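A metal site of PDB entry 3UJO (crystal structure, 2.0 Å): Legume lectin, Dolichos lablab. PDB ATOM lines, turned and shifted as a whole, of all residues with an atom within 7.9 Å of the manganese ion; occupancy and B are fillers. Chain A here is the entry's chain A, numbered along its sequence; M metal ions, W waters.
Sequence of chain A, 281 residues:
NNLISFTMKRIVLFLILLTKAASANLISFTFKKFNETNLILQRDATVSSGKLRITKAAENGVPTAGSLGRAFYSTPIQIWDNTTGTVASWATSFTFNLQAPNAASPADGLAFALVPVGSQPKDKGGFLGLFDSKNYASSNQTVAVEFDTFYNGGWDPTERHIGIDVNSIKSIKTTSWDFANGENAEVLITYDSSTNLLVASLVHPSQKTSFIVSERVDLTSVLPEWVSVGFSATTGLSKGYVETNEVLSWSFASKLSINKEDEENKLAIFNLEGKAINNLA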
ATOM      1  N   GLY A 126      28.188  12.371   3.190  1.00  0.00           N
ATOM      2  CA  GLY A 126      27.417  12.535   4.428  1.00  0.00           C
ATOM      3  C   GLY A 126      28.102  11.972   5.653  1.00  0.00           C
ATOM      4  O   GLY A 126      27.915  12.483   6.762  1.00  0.00           O
ATOM      5  N   LEU A 128      31.220  12.098   6.153  1.00  0.00           N
ATOM      6  CA  LEU A 128      32.332  13.030   6.417  1.00  0.00           C
ATOM      7  C   LEU A 128      33.716  12.377   6.503  1.00  0.00           C
ATOM      8  O   LEU A 128      34.634  12.940   7.102  1.00  0.00           O
ATOM      9  CB  LEU A 128      32.043  13.879   7.669  1.00  0.00           C
ATOM     10  CG  LEU A 128      30.933  14.928   7.621  1.00  0.00           C
ATOM     11  CD1 LEU A 128      30.476  15.289   9.030  1.00  0.00           C
ATOM     12  CD2 LEU A 128      31.350  16.171   6.852  1.00  0.00           C
ATOM     13  N   GLU A 146      31.757  18.597  14.217  1.00  0.00           N
ATOM     14  CA  GLU A 146      31.407  18.959  12.838  1.00  0.00           C
ATOM     15  C   GLU A 146      31.064  20.439  12.666  1.00  0.00           C
ATOM     16  O   GLU A 146      30.626  21.110  13.599  1.00  0.00           O
ATOM     17  CB  GLU A 146      30.253  18.087  12.322  1.00  0.00           C
ATOM     18  CG  GLU A 146      28.923  18.274  13.052  1.00  0.00           C
ATOM     19  CD  GLU A 146      27.892  17.216  12.714  1.00  0.00           C
ATOM     20  OE1 GLU A 146      28.061  16.506  11.687  1.00  0.00           O
ATOM     21  OE2 GLU A 146      26.902  17.085  13.467  1.00  0.00           O
ATOM     22  N   PHE A 147      31.274  20.937  11.451  1.00  0.00           N
ATOM     23  CA  PHE A 147      30.853  22.273  11.053  1.00  0.00           C
ATOM     24  C   PHE A 147      30.014  22.126   9.784  1.00  0.00           C
ATOM     25  O   PHE A 147      30.433  22.526   8.690  1.00  0.00           O
ATOM     26  CB  PHE A 147      32.058  23.196  10.845  1.00  0.00           C
ATOM     27  CG  PHE A 147      32.993  23.253  12.037  1.00  0.00           C
ATOM     28  CD1 PHE A 147      32.704  24.070  13.121  1.00  0.00           C
ATOM     29  CD2 PHE A 147      34.144  22.478  12.061  1.00  0.00           C
ATOM     30  CE1 PHE A 147      33.570  24.135  14.222  1.00  0.00           C
ATOM     31  CE2 PHE A 147      35.008  22.514  13.161  1.00  0.00           C
ATOM     32  CZ  PHE A 147      34.720  23.346  14.245  1.00  0.00           C
ATOM     33  N   ASP A 148      28.828  21.557   9.956  1.00  0.00           N
ATOM     34  CA  ASP A 148      27.966  21.109   8.868  1.00  0.00           C
ATOM     35  C   ASP A 148      27.449  22.246   7.983  1.00  0.00           C
ATOM     36  O   ASP A 148      27.304  23.388   8.440  1.00  0.00           O
ATOM     37  CB  ASP A 148      26.791  20.316   9.437  1.00  0.00           C
ATOM     38  CG  ASP A 148      26.318  19.222   8.508  1.00  0.00           C
ATOM     39  OD1 ASP A 148      26.165  19.472   7.291  1.00  0.00           O
ATOM     40  OD2 ASP A 148      26.088  18.099   9.005  1.00  0.00           O
ATOM     41  N   THR A 149      27.186  21.924   6.719  1.00  0.00           N
ATOM     42  CA  THR A 149      26.689  22.899   5.743  1.00  0.00           C
ATOM     43  C   THR A 149      25.537  22.347   4.893  1.00  0.00           C
ATOM     44  O   THR A 149      24.692  23.102   4.416  1.00  0.00           O
ATOM     45  CB  THR A 149      27.805  23.395   4.791  1.00  0.00           C
ATOM     46  OG1 THR A 149      28.261  22.315   3.970  1.00  0.00           O
ATOM     47  CG2 THR A 149      28.985  23.967   5.583  1.00  0.00           C
ATOM     48  N   PHE A 150      25.515  21.027   4.697  1.00  0.00           N
ATOM     49  CA  PHE A 150      24.500  20.393   3.853  1.00  0.00           C
ATOM     50  C   PHE A 150      23.376  19.738   4.663  1.00  0.00           C
ATOM     51  O   PHE A 150      23.610  19.243   5.769  1.00  0.00           O
ATOM     52  CB  PHE A 150      25.142  19.380   2.899  1.00  0.00           C
ATOM     53  CG  PHE A 150      24.268  19.013   1.729  1.00  0.00           C
ATOM     54  CD1 PHE A 150      23.563  17.814   1.718  1.00  0.00           C
ATOM     55  CD2 PHE A 150      24.142  19.875   0.646  1.00  0.00           C
ATOM     56  CE1 PHE A 150      22.753  17.476   0.630  1.00  0.00           C
ATOM     57  CE2 PHE A 150      23.334  19.544  -0.448  1.00  0.00           C
ATOM     58  CZ  PHE A 150      22.636  18.344  -0.443  1.00  0.00           C
ATOM     59  N   ASN A 152      20.976  16.769   5.137  1.00  0.00           N
ATOM     60  CA  ASN A 152      20.687  15.366   4.863  1.00  0.00           C
ATOM     61  C   ASN A 152      19.461  14.911   5.654  1.00  0.00           C
ATOM     62  O   ASN A 152      18.456  14.497   5.078  1.00  0.00           O
ATOM     63  CB  ASN A 152      21.887  14.473   5.170  1.00  0.00           C
ATOM     64  CG  ASN A 152      23.113  14.843   4.349  1.00  0.00           C
ATOM     65  OD1 ASN A 152      23.603  15.973   4.404  1.00  0.00           O
ATOM     66  ND2 ASN A 152      23.633  13.877   3.597  1.00  0.00           N
ATOM     67  N   GLY A 153      19.561  14.981   6.983  1.00  0.00           N
ATOM     68  CA  GLY A 153      18.430  14.708   7.867  1.00  0.00           C
ATOM     69  C   GLY A 153      18.294  13.287   8.379  1.00  0.00           C
ATOM     70  O   GLY A 153      17.778  13.072   9.470  1.00  0.00           O
ATOM     71  N   TRP A 155      20.463  11.472   9.466  1.00  0.00           N
ATOM     72  CA  TRP A 155      21.289  11.395  10.673  1.00  0.00           C
ATOM     73  C   TRP A 155      21.539  12.808  11.215  1.00  0.00           C
ATOM     74  O   TRP A 155      22.309  12.990  12.167  1.00  0.00           O
ATOM     75  CB  TRP A 155      22.617  10.686  10.364  1.00  0.00           C
ATOM     76  CG  TRP A 155      23.311  11.202   9.132  1.00  0.00           C
ATOM     77  CD1 TRP A 155      24.174  12.256   9.044  1.00  0.00           C
ATOM     78  CD2 TRP A 155      23.184  10.680   7.793  1.00  0.00           C
ATOM     79  NE1 TRP A 155      24.595  12.419   7.745  1.00  0.00           N
ATOM     80  CE2 TRP A 155      24.004  11.473   6.961  1.00  0.00           C
ATOM     81  CE3 TRP A 155      22.472   9.617   7.232  1.00  0.00           C
ATOM     82  CZ2 TRP A 155      24.129  11.230   5.588  1.00  0.00           C
ATOM     83  CZ3 TRP A 155      22.586   9.381   5.864  1.00  0.00           C
ATOM     84  CH2 TRP A 155      23.409  10.187   5.062  1.00  0.00           C
ATOM     85  N   ASP A 156      20.860  13.787  10.615  1.00  0.00           N
ATOM     86  CA  ASP A 156      21.069  15.203  10.919  1.00  0.00           C
ATOM     87  C   ASP A 156      19.793  15.888  11.418  1.00  0.00           C
ATOM     88  O   ASP A 156      18.690  15.387  11.181  1.00  0.00           O
ATOM     89  CB  ASP A 156      21.600  15.924   9.667  1.00  0.00           C
ATOM     90  CG  ASP A 156      23.010  15.501   9.300  1.00  0.00           C
ATOM     91  OD1 ASP A 156      23.900  15.512  10.174  1.00  0.00           O
ATOM     92  OD2 ASP A 156      23.232  15.159   8.114  1.00  0.00           O
ATOM     93  N   PRO A 157      19.942  17.028  12.129  1.00  0.00           N
ATOM     94  CA  PRO A 157      18.806  17.831  12.607  1.00  0.00           C
ATOM     95  C   PRO A 157      18.101  18.641  11.502  1.00  0.00           C
ATOM     96  O   PRO A 157      17.771  18.092  10.453  1.00  0.00           O
ATOM     97  CB  PRO A 157      19.442  18.767  13.651  1.00  0.00           C
ATOM     98  CG  PRO A 157      20.739  18.128  13.993  1.00  0.00           C
ATOM     99  CD  PRO A 157      21.202  17.485  12.737  1.00  0.00           C
ATOM    100  N   GLU A 159      18.893  22.161  10.150  1.00  0.00           N
ATOM    101  CA  GLU A 159      19.652  22.998   9.207  1.00  0.00           C
ATOM    102  C   GLU A 159      21.158  22.941   9.461  1.00  0.00           C
ATOM    103  O   GLU A 159      21.705  21.867   9.747  1.00  0.00           O
ATOM    104  CB  GLU A 159      19.130  24.452   9.229  1.00  0.00           C
ATOM    105  CG  GLU A 159      19.001  25.071  10.625  1.00  0.00           C
ATOM    106  CD  GLU A 159      18.697  26.558  10.581  1.00  0.00           C
ATOM    107  OE1 GLU A 159      19.448  27.303   9.914  1.00  0.00           O
ATOM    108  OE2 GLU A 159      17.718  26.982  11.238  1.00  0.00           O
ATOM    109  N   HIS A 161      24.472  23.202  11.499  1.00  0.00           N
ATOM    110  CA  HIS A 161      24.694  22.856  12.895  1.00  0.00           C
ATOM    111  C   HIS A 161      26.152  22.537  13.244  1.00  0.00           C
ATOM    112  O   HIS A 161      26.867  21.926  12.458  1.00  0.00           O
ATOM    113  CB  HIS A 161      23.799  21.668  13.295  1.00  0.00           C
ATOM    114  CG  HIS A 161      23.974  20.456  12.428  1.00  0.00           C
ATOM    115  ND1 HIS A 161      23.246  20.269  11.275  1.00  0.00           N
ATOM    116  CD2 HIS A 161      24.785  19.388  12.543  1.00  0.00           C
ATOM    117  CE1 HIS A 161      23.606  19.126  10.714  1.00  0.00           C
ATOM    118  NE2 HIS A 161      24.533  18.571  11.462  1.00  0.00           N
ATOM    119  N   ILE A 162      26.558  22.970  14.437  1.00  0.00           N
ATOM    120  CA  ILE A 162      27.829  22.561  15.029  1.00  0.00           C
ATOM    121  C   ILE A 162      27.529  21.506  16.085  1.00  0.00           C
ATOM    122  O   ILE A 162      26.871  21.802  17.097  1.00  0.00           O
ATOM    123  CB  ILE A 162      28.593  23.738  15.670  1.00  0.00           C
ATOM    124  CG1 ILE A 162      28.749  24.908  14.686  1.00  0.00           C
ATOM    125  CG2 ILE A 162      29.963  23.280  16.185  1.00  0.00           C
ATOM    126  CD1 ILE A 162      29.215  26.202  15.314  1.00  0.00           C
ATOM    127  N   GLY A 163      27.989  20.283  15.865  1.00  0.00           N
ATOM    128  CA  GLY A 163      27.702  19.175  16.778  1.00  0.00           C
ATOM    129  C   GLY A 163      28.819  18.165  16.931  1.00  0.00           C
ATOM    130  O   GLY A 163      29.855  18.249  16.263  1.00  0.00           O
ATOM    131  N   ILE A 164      28.590  17.209  17.831  1.00  0.00           N
ATOM    132  CA  ILE A 164      29.554  16.145  18.111  1.00  0.00           C
ATOM    133  C   ILE A 164      29.042  14.825  17.529  1.00  0.00           C
ATOM    134  O   ILE A 164      27.844  14.536  17.604  1.00  0.00           O
ATOM    135  CB  ILE A 164      29.812  15.984  19.627  1.00  0.00           C
ATOM    136  CG1 ILE A 164      29.808  17.350  20.328  1.00  0.00           C
ATOM    137  CG2 ILE A 164      31.124  15.240  19.877  1.00  0.00           C
ATOM    138  CD1 ILE A 164      29.493  17.293  21.810  1.00  0.00           C
ATOM    139  N   ASP A 165      29.945  14.043  16.960  1.00  0.00           N
ATOM    140  CA  ASP A 165      29.601  12.738  16.379  1.00  0.00           C
ATOM    141  C   ASP A 165      30.143  11.607  17.249  1.00  0.00           C
ATOM    142  O   ASP A 165      31.353  11.414  17.358  1.00  0.00           O
ATOM    143  CB  ASP A 165      30.127  12.627  14.945  1.00  0.00           C
ATOM    144  CG  ASP A 165      29.705  13.813  14.071  1.00  0.00           C
ATOM    145  OD1 ASP A 165      28.641  14.410  14.325  1.00  0.00           O
ATOM    146  OD2 ASP A 165      30.462  14.138  13.125  1.00  0.00           O
ATOM    147  N   ILE A 169      27.675   8.720  12.642  1.00  0.00           N
ATOM    148  CA  ILE A 169      27.391  10.022  12.032  1.00  0.00           C
ATOM    149  C   ILE A 169      26.086  10.631  12.573  1.00  0.00           C
ATOM    150  O   ILE A 169      25.802  11.817  12.350  1.00  0.00           O
ATOM    151  CB  ILE A 169      27.400   9.914  10.475  1.00  0.00           C
ATOM    152  CG1 ILE A 169      27.589  11.286   9.823  1.00  0.00           C
ATOM    153  CG2 ILE A 169      26.168   9.183   9.946  1.00  0.00           C
ATOM    154  CD1 ILE A 169      28.994  11.864   9.965  1.00  0.00           C
ATOM    155  N   LYS A 170      25.307   9.824  13.284  1.00  0.00           N
ATOM    156  CA  LYS A 170      24.015  10.233  13.828  1.00  0.00           C
ATOM    157  C   LYS A 170      24.193  10.877  15.210  1.00  0.00           C
ATOM    158  O   LYS A 170      24.620  10.228  16.162  1.00  0.00           O
ATOM    159  CB  LYS A 170      23.074   9.029  13.923  1.00  0.00           C
ATOM    160  CG  LYS A 170      21.600   9.374  13.958  1.00  0.00           C
ATOM    161  CD  LYS A 170      20.746   8.117  13.907  1.00  0.00           C
ATOM    162  CE  LYS A 170      19.265   8.444  13.844  1.00  0.00           C
ATOM    163  NZ  LYS A 170      18.865   9.022  12.526  1.00  0.00           N
ATOM    164  N   SER A 171      23.846  12.166  15.300  1.00  0.00           N
ATOM    165  CA  SER A 171      23.981  12.938  16.533  1.00  0.00           C
ATOM    166  C   SER A 171      22.768  12.785  17.453  1.00  0.00           C
ATOM    167  O   SER A 171      21.716  12.306  17.032  1.00  0.00           O
ATOM    168  CB  SER A 171      24.215  14.411  16.215  1.00  0.00           C
ATOM    169  OG  SER A 171      25.428  14.609  15.506  1.00  0.00           O
ATOM    170  N   THR A 174      22.727  18.783  19.119  1.00  0.00           N
ATOM    171  CA  THR A 174      23.566  19.784  18.440  1.00  0.00           C
ATOM    172  C   THR A 174      23.066  21.192  18.754  1.00  0.00           C
ATOM    173  O   THR A 174      22.126  21.368  19.536  1.00  0.00           O
ATOM    174  CB  THR A 174      23.560  19.576  16.908  1.00  0.00           C
ATOM    175  OG1 THR A 174      22.227  19.683  16.408  1.00  0.00           O
ATOM    176  CG2 THR A 174      24.135  18.213  16.520  1.00  0.00           C
HETATM  177 MN    MN M   1      25.448  16.271  11.086  1.00  0.00          MN
HETATM  178 CA    CA M   2      25.876  16.291   6.898  1.00  0.00          CA
HETATM  179  O   HOH W   1      26.231  14.051  10.808  1.00  0.00           O
HETATM  180  O   HOH W   2      24.975  14.997  12.959  1.00  0.00           O
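NE1 of Trp 155 is in hydrogen-bond range of OD2 of Asp 156, at 3.1 Å.
The backbone carbonyl oxygen (O) of Gly 163 lies within hydrogen-bond range of the backbone NH (N) of Glu 146, 2.8 Å away.
The backbone NH (N) of Phe 150 lies within hydrogen-bond range of the side-chain carboxylate (OD1) of Asp 148, 3.1 Å away.
O of Glu 159 lies within hydrogen-bond range of ND1 of His 161 (2.7 Å).
The backbone carbonyl oxygen (O) of His 161 is in hydrogen-bond range of the backbone NH (N) of Asp 148, 3.2 Å away.
The manganese ion is bound by OD1 of Asp 156, water W2, water W1, NE2 of His 161 and OE1 of Glu 146.
The manganese ion has five donor atoms within binding distance.
Slightly farther from the manganese ion lies OD2 of Asp 148 (2.8 Å).
Slightly farther from the manganese ion lies the side-chain carboxylate (OE2) of Glu 146 (2.9 Å).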
